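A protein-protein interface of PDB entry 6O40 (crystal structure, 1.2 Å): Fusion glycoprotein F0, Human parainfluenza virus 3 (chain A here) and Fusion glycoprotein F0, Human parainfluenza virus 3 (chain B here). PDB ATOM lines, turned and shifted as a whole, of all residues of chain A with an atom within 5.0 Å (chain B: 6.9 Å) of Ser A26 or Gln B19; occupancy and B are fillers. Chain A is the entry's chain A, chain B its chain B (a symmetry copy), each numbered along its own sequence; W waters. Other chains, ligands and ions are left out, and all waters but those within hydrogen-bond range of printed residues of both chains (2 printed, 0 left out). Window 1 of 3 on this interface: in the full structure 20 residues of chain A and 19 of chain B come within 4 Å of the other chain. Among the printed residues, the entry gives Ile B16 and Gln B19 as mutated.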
ATOM      1  N   GLN A  22      10.829  -5.569  16.858  1.00  0.00           N
ATOM      2  CA  GLN A  22      10.622  -6.883  17.462  1.00  0.00           C
ATOM      3  C   GLN A  22       9.804  -6.791  18.731  1.00  0.00           C
ATOM      4  O   GLN A  22       8.969  -7.665  18.985  1.00  0.00           O
ATOM      5  CB  GLN A  22      11.955  -7.561  17.735  1.00  0.00           C
ATOM      6  CG  GLN A  22      12.656  -7.952  16.487  1.00  0.00           C
ATOM      7  CD  GLN A  22      13.891  -8.768  16.755  1.00  0.00           C
ATOM      8  OE1 GLN A  22      14.786  -8.335  17.464  1.00  0.00           O
ATOM      9  NE2 GLN A  22      13.942  -9.964  16.188  1.00  0.00           N
ATOM     10  N   SER A  23      10.022  -5.760  19.540  1.00  0.00           N
ATOM     11  CA  SER A  23       9.197  -5.610  20.742  1.00  0.00           C
ATOM     12  C   SER A  23       7.751  -5.318  20.375  1.00  0.00           C
ATOM     13  O   SER A  23       6.827  -5.832  21.017  1.00  0.00           O
ATOM     14  CB  SER A  23       9.742  -4.512  21.640  1.00  0.00           C
ATOM     15  OG  SER A  23      10.957  -4.938  22.271  1.00  0.00           O
ATOM     16  N   VAL A  24       7.514  -4.492  19.359  1.00  0.00           N
ATOM     17  CA  VAL A  24       6.155  -4.286  18.849  1.00  0.00           C
ATOM     18  C   VAL A  24       5.553  -5.586  18.346  1.00  0.00           C
ATOM     19  O   VAL A  24       4.367  -5.850  18.557  1.00  0.00           O
ATOM     20  CB  VAL A  24       6.193  -3.191  17.756  1.00  0.00           C
ATOM     21  CG1 VAL A  24       5.039  -3.313  16.785  1.00  0.00           C
ATOM     22  CG2 VAL A  24       6.256  -1.778  18.365  1.00  0.00           C
ATOM     23  N   GLN A  25       6.358  -6.422  17.701  1.00  0.00           N
ATOM     24  CA  GLN A  25       5.885  -7.732  17.186  1.00  0.00           C
ATOM     25  C   GLN A  25       5.415  -8.583  18.370  1.00  0.00           C
ATOM     26  O   GLN A  25       4.371  -9.217  18.255  1.00  0.00           O
ATOM     27  CB  GLN A  25       6.982  -8.417  16.373  1.00  0.00           C
ATOM     28  CG  GLN A  25       7.179  -7.796  14.996  1.00  0.00           C
ATOM     29  CD  GLN A  25       8.482  -8.212  14.360  1.00  0.00           C
ATOM     30  OE1 GLN A  25       9.318  -8.847  14.984  1.00  0.00           O
ATOM     31  NE2 GLN A  25       8.658  -7.854  13.105  1.00  0.00           N
ATOM     32  N   SER A  26       6.159  -8.590  19.475  1.00  0.00           N
ATOM     33  CA  SER A  26       5.778  -9.342  20.700  1.00  0.00           C
ATOM     34  C   SER A  26       4.443  -8.799  21.220  1.00  0.00           C
ATOM     35  O   SER A  26       3.565  -9.588  21.539  1.00  0.00           O
ATOM     36  CB  SER A  26       6.858  -9.265  21.740  1.00  0.00           C
ATOM     37  OG  SER A  26       8.012  -9.964  21.298  1.00  0.00           O
ATOM     38  N   SER A  27       4.304  -7.479  21.303  1.00  0.00           N
ATOM     39  CA  SER A  27       3.068  -6.802  21.762  1.00  0.00           C
ATOM     40  C   SER A  27       1.886  -7.289  20.923  1.00  0.00           C
ATOM     41  O   SER A  27       0.849  -7.622  21.488  1.00  0.00           O
ATOM     42  CB  SER A  27       3.191  -5.313  21.653  1.00  0.00           C
ATOM     43  OG  SER A  27       3.973  -4.788  22.707  1.00  0.00           O
ATOM     44  N   ILE A  28       2.033  -7.279  19.601  1.00  0.00           N
ATOM     45  CA  ILE A  28       0.944  -7.674  18.663  1.00  0.00           C
ATOM     46  C   ILE A  28       0.618  -9.147  18.887  1.00  0.00           C
ATOM     47  O   ILE A  28      -0.569  -9.478  18.912  1.00  0.00           O
ATOM     48  CB  ILE A  28       1.315  -7.353  17.207  1.00  0.00           C
ATOM     49  CG1 ILE A  28       1.292  -5.842  16.986  1.00  0.00           C
ATOM     50  CG2 ILE A  28       0.401  -8.090  16.237  1.00  0.00           C
ATOM     51  CD1 ILE A  28       1.964  -5.404  15.718  1.00  0.00           C
ATOM     52  N   GLY A  29       1.617 -10.003  19.062  1.00  0.00           N
ATOM     53  CA  GLY A  29       1.319 -11.406  19.338  1.00  0.00           C
ATOM     54  C   GLY A  29       0.454 -11.594  20.577  1.00  0.00           C
ATOM     55  O   GLY A  29      -0.475 -12.411  20.591  1.00  0.00           O
ATOM     56  N   ASN A  30       0.723 -10.820  21.627  1.00  0.00           N
ATOM     57  CA  ASN A  30      -0.089 -10.915  22.843  1.00  0.00           C
ATOM     58  C   ASN A  30      -1.424 -10.216  22.695  1.00  0.00           C
ATOM     59  O   ASN A  30      -2.397 -10.632  23.335  1.00  0.00           O
ATOM     60  CB  ASN A  30       0.726 -10.411  24.015  1.00  0.00           C
ATOM     61  CG  ASN A  30       1.698 -11.441  24.493  1.00  0.00           C
ATOM     62  OD1 ASN A  30       1.345 -12.623  24.610  1.00  0.00           O
ATOM     63  ND2 ASN A  30       2.925 -11.037  24.757  1.00  0.00           N
ATOM     64  N   ASN B  14      -0.434  -6.878  30.802  1.00  0.00           N
ATOM     65  CA  ASN B  14       0.772  -6.251  31.398  1.00  0.00           C
ATOM     66  C   ASN B  14       1.982  -6.595  30.515  1.00  0.00           C
ATOM     67  O   ASN B  14       2.844  -5.741  30.376  1.00  0.00           O
ATOM     68  CB  ASN B  14       0.865  -6.565  32.894  1.00  0.00           C
ATOM     69  CG  ASN B  14      -0.131  -5.751  33.703  1.00  0.00           C
ATOM     70  OD1 ASN B  14      -0.187  -4.524  33.600  1.00  0.00           O
ATOM     71  ND2 ASN B  14      -0.945  -6.419  34.499  1.00  0.00           N
ATOM     72  N   LYS B  15       2.021  -7.778  29.901  1.00  0.00           N
ATOM     73  CA  LYS B  15       3.133  -8.169  28.994  1.00  0.00           C
ATOM     74  C   LYS B  15       3.083  -7.273  27.750  1.00  0.00           C
ATOM     75  O   LYS B  15       4.137  -6.841  27.304  1.00  0.00           O
ATOM     76  CB  LYS B  15       3.067  -9.644  28.593  1.00  0.00           C
ATOM     77  CG  LYS B  15       4.357 -10.202  28.006  1.00  0.00           C
ATOM     78  CD  LYS B  15       5.606  -9.787  28.762  1.00  0.00           C
ATOM     79  CE  LYS B  15       6.857 -10.517  28.324  1.00  0.00           C
ATOM     80  NZ  LYS B  15       6.842 -10.803  26.874  1.00  0.00           N
ATOM     81  N   ILE B  16       1.895  -7.006  27.211  1.00  0.00           N
ATOM     82  CA  ILE B  16       1.745  -6.129  26.017  1.00  0.00           C
ATOM     83  C   ILE B  16       2.335  -4.764  26.374  1.00  0.00           C
ATOM     84  O   ILE B  16       3.109  -4.227  25.584  1.00  0.00           O
ATOM     85  CB  ILE B  16       0.273  -6.006  25.569  1.00  0.00           C
ATOM     86  CG1 ILE B  16      -0.307  -7.358  25.151  1.00  0.00           C
ATOM     87  CG2 ILE B  16       0.132  -4.968  24.462  1.00  0.00           C
ATOM     88  CD1 ILE B  16      -1.805  -7.360  24.988  1.00  0.00           C
ATOM     89  N   LYS B  17       1.998  -4.241  27.552  1.00  0.00           N
ATOM     90  CA  LYS B  17       2.457  -2.900  27.987  1.00  0.00           C
ATOM     91  C   LYS B  17       3.975  -2.875  28.201  1.00  0.00           C
ATOM     92  O   LYS B  17       4.603  -1.925  27.751  1.00  0.00           O
ATOM     93  CB  LYS B  17       1.754  -2.468  29.275  1.00  0.00           C
ATOM     94  CG  LYS B  17       2.107  -1.064  29.727  1.00  0.00           C
ATOM     95  CD  LYS B  17       1.199  -0.550  30.808  1.00  0.00           C
ATOM     96  CE  LYS B  17      -0.051   0.101  30.269  1.00  0.00           C
ATOM     97  NZ  LYS B  17      -0.810   0.777  31.343  1.00  0.00           N
ATOM     98  N   SER B  18       4.521  -3.907  28.836  1.00  0.00           N
ATOM     99  CA  SER B  18       5.967  -4.033  29.136  1.00  0.00           C
ATOM    100  C   SER B  18       6.764  -4.044  27.828  1.00  0.00           C
ATOM    101  O   SER B  18       7.805  -3.391  27.764  1.00  0.00           O
ATOM    102  CB  SER B  18       6.228  -5.269  29.956  1.00  0.00           C
ATOM    103  OG  SER B  18       7.592  -5.355  30.310  1.00  0.00           O
ATOM    104  N   GLN B  19       6.272  -4.753  26.814  1.00  0.00           N
ATOM    105  CA  GLN B  19       6.975  -4.872  25.512  1.00  0.00           C
ATOM    106  C   GLN B  19       6.863  -3.546  24.761  1.00  0.00           C
ATOM    107  O   GLN B  19       7.823  -3.174  24.095  1.00  0.00           O
ATOM    108  CB  GLN B  19       6.472  -6.084  24.733  1.00  0.00           C
ATOM    109  CG  GLN B  19       7.206  -7.361  25.123  1.00  0.00           C
ATOM    110  CD  GLN B  19       8.709  -7.205  25.027  1.00  0.00           C
ATOM    111  OE1 GLN B  19       9.284  -7.171  23.945  1.00  0.00           O
ATOM    112  NE2 GLN B  19       9.363  -7.064  26.169  1.00  0.00           N
ATOM    113  N   LEU B  20       5.739  -2.855  24.891  1.00  0.00           N
ATOM    114  CA  LEU B  20       5.565  -1.520  24.278  1.00  0.00           C
ATOM    115  C   LEU B  20       6.604  -0.584  24.909  1.00  0.00           C
ATOM    116  O   LEU B  20       7.268   0.145  24.179  1.00  0.00           O
ATOM    117  CB  LEU B  20       4.137  -1.039  24.532  1.00  0.00           C
ATOM    118  CG  LEU B  20       3.839   0.372  24.049  1.00  0.00           C
ATOM    119  CD1 LEU B  20       4.046   0.468  22.548  1.00  0.00           C
ATOM    120  CD2 LEU B  20       2.423   0.777  24.422  1.00  0.00           C
ATOM    121  N   GLU B  21       6.784  -0.652  26.230  1.00  0.00           N
ATOM    122  CA  GLU B  21       7.753   0.220  26.946  1.00  0.00           C
ATOM    123  C   GLU B  21       9.184  -0.118  26.489  1.00  0.00           C
ATOM    124  O   GLU B  21       9.962   0.813  26.285  1.00  0.00           O
ATOM    125  CB  GLU B  21       7.490   0.125  28.451  1.00  0.00           C
ATOM    126  CG  GLU B  21       6.183   0.807  28.832  1.00  0.00           C
ATOM    127  CD  GLU B  21       5.555   0.442  30.169  1.00  0.00           C
ATOM    128  OE1 GLU B  21       6.015  -0.508  30.806  1.00  0.00           O
ATOM    129  OE2 GLU B  21       4.585   1.116  30.547  1.00  0.00           O
ATOM    130  N   GLU B  22       9.519  -1.390  26.295  1.00  0.00           N
ATOM    131  CA  GLU B  22      10.863  -1.784  25.796  1.00  0.00           C
ATOM    132  C   GLU B  22      11.059  -1.207  24.386  1.00  0.00           C
ATOM    133  O   GLU B  22      12.142  -0.717  24.088  1.00  0.00           O
ATOM    134  CB  GLU B  22      11.042  -3.302  25.765  1.00  0.00           C
ATOM    135  CG  GLU B  22      12.463  -3.704  25.410  1.00  0.00           C
ATOM    136  CD  GLU B  22      12.762  -5.193  25.414  1.00  0.00           C
ATOM    137  OE1 GLU B  22      12.156  -5.898  26.227  1.00  0.00           O
ATOM    138  OE2 GLU B  22      13.602  -5.636  24.594  1.00  0.00           O
ATOM    139  N   SER B  23      10.030  -1.279  23.543  1.00  0.00           N
ATOM    140  CA  SER B  23      10.064  -0.764  22.154  1.00  0.00           C
ATOM    141  C   SER B  23      10.428   0.723  22.182  1.00  0.00           C
ATOM    142  O   SER B  23      11.263   1.143  21.376  1.00  0.00           O
ATOM    143  CB  SER B  23       8.756  -0.998  21.451  1.00  0.00           C
ATOM    144  OG  SER B  23       8.842  -0.615  20.091  1.00  0.00           O
ATOM    145  N   LYS B  24       9.827   1.493  23.088  1.00  0.00           N
ATOM    146  CA  LYS B  24      10.091   2.926  23.179  1.00  0.00           C
ATOM    147  C   LYS B  24      11.529   3.199  23.588  1.00  0.00           C
ATOM    148  O   LYS B  24      12.169   4.127  23.062  1.00  0.00           O
ATOM    149  CB  LYS B  24       9.107   3.546  24.181  1.00  0.00           C
ATOM    150  CG  LYS B  24       7.682   3.547  23.678  1.00  0.00           C
ATOM    151  CD  LYS B  24       6.733   4.178  24.691  1.00  0.00           C
ATOM    152  CE  LYS B  24       5.269   4.012  24.262  1.00  0.00           C
ATOM    153  NZ  LYS B  24       4.310   4.510  25.286  1.00  0.00           N
ATOM    154  N   TRP B  26      14.145   1.219  22.837  1.00  0.00           N
ATOM    155  CA  TRP B  26      15.001   0.964  21.679  1.00  0.00           C
ATOM    156  C   TRP B  26      14.968   2.123  20.688  1.00  0.00           C
ATOM    157  O   TRP B  26      16.001   2.466  20.119  1.00  0.00           O
ATOM    158  CB  TRP B  26      14.605  -0.350  21.003  1.00  0.00           C
ATOM    159  CG  TRP B  26      14.986  -1.596  21.748  1.00  0.00           C
ATOM    160  CD1 TRP B  26      14.151  -2.542  22.254  1.00  0.00           C
ATOM    161  CD2 TRP B  26      16.319  -2.023  22.055  1.00  0.00           C
ATOM    162  NE1 TRP B  26      14.880  -3.546  22.862  1.00  0.00           N
ATOM    163  CE2 TRP B  26      16.215  -3.258  22.738  1.00  0.00           C
ATOM    164  CE3 TRP B  26      17.591  -1.492  21.809  1.00  0.00           C
ATOM    165  CZ2 TRP B  26      17.338  -3.961  23.207  1.00  0.00           C
ATOM    166  CZ3 TRP B  26      18.706  -2.200  22.272  1.00  0.00           C
ATOM    167  CH2 TRP B  26      18.565  -3.414  22.966  1.00  0.00           C
HETATM  168  O   HOH W   1      13.246  -6.486  21.236  1.00  0.00           O
HETATM  169  O   HOH W   2       5.159 -13.053  25.626  1.00  0.00           O
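OE1 of Gln B19 lies within hydrogen-bond range of OG of Ser A23 (3.3 Å). O of Ile B16 lies within hydrogen-bond range of OG of Ser A27, 3.1 Å away. The side-chain hydroxyl (OG) of Ser A27 sits at hydrogen-bond distance from the backbone NH (N) of Leu B20 (3.4 Å).
The side-chain amide nitrogen (NE2) of Gln B19 sits at hydrogen-bond distance from the side-chain carboxylate (OE1) of Glu B22 (3.0 Å). OE2 of Glu B22 sits at hydrogen-bond distance from NE1 of Trp B26 (3.0 Å). OG of Ser A26 is in hydrogen-bond range of O of Gln A22. OG of Ser A27 sits at hydrogen-bond distance from O of Ser A23, at 3.5 Å.
Among the printed residues, pairs that only touch across the chains: Ser A23 with Glu B22, Ser A23 with Ser B23, Ser A23 with Trp B26, Val A24 with Ser B23, Ser A26 with Gln B19, Ser A27 with Gln B19, Asn A30 with Lys B15 and Asn A30 with Ile B16.
Ser A26 touches one residue of chain B. Gln B19 touches just these residues of chain A: Ser A23 (3.3 Å), Ser A26 (3.9 Å) and Ser A27 (3.5 Å). Printed residues of chain A within 4 Å of Ser B23: Ser A23 and Val A24. Of the printed residues of chain B, Ser A23 touches Gln B19, Glu B22, Ser B23 and Trp B26. Printed residues of chain B within 4 Å of Val A24: Ser B23. Printed residues of chain A within 4 Å of Glu B22: Ser A23. Of the printed residues of chain B, Ser A27 touches Ile B16, Gln B19 and Leu B20. Ser B18 touches none of the printed residues of chain A. The nearest residue of chain B that does not touch Ser A26 is Lys B15 (5.4 Å). The nearest printed residue of chain B that does not touch Ser A23 is Leu B20 (5.0 Å).
Hydrophobic or aromatic side chains of chain B that line the printed part of chain A: Ile B16 and Trp B26. Of the 9 printed residues of chain A, 5 touch a printed residue of chain B. Hydrophobic or aromatic side chains of chain A within 4 Å of the printed part of chain B: Val A24. Among the printed residues, no Asp or Glu carboxylate lies within 4 Å of a Lys or Arg side-chain nitrogen of the other chain.
Water W1 bridges the side-chain hydroxyl (OG) of Ser A23 (3.0 Å) and the side-chain carboxylate (OE2) of Glu B22 (3.5 Å). Water W2 lies within hydrogen-bond range of NZ of Lys B15 (3.1 Å) and ND2 of Asn A30 (3.1 Å).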
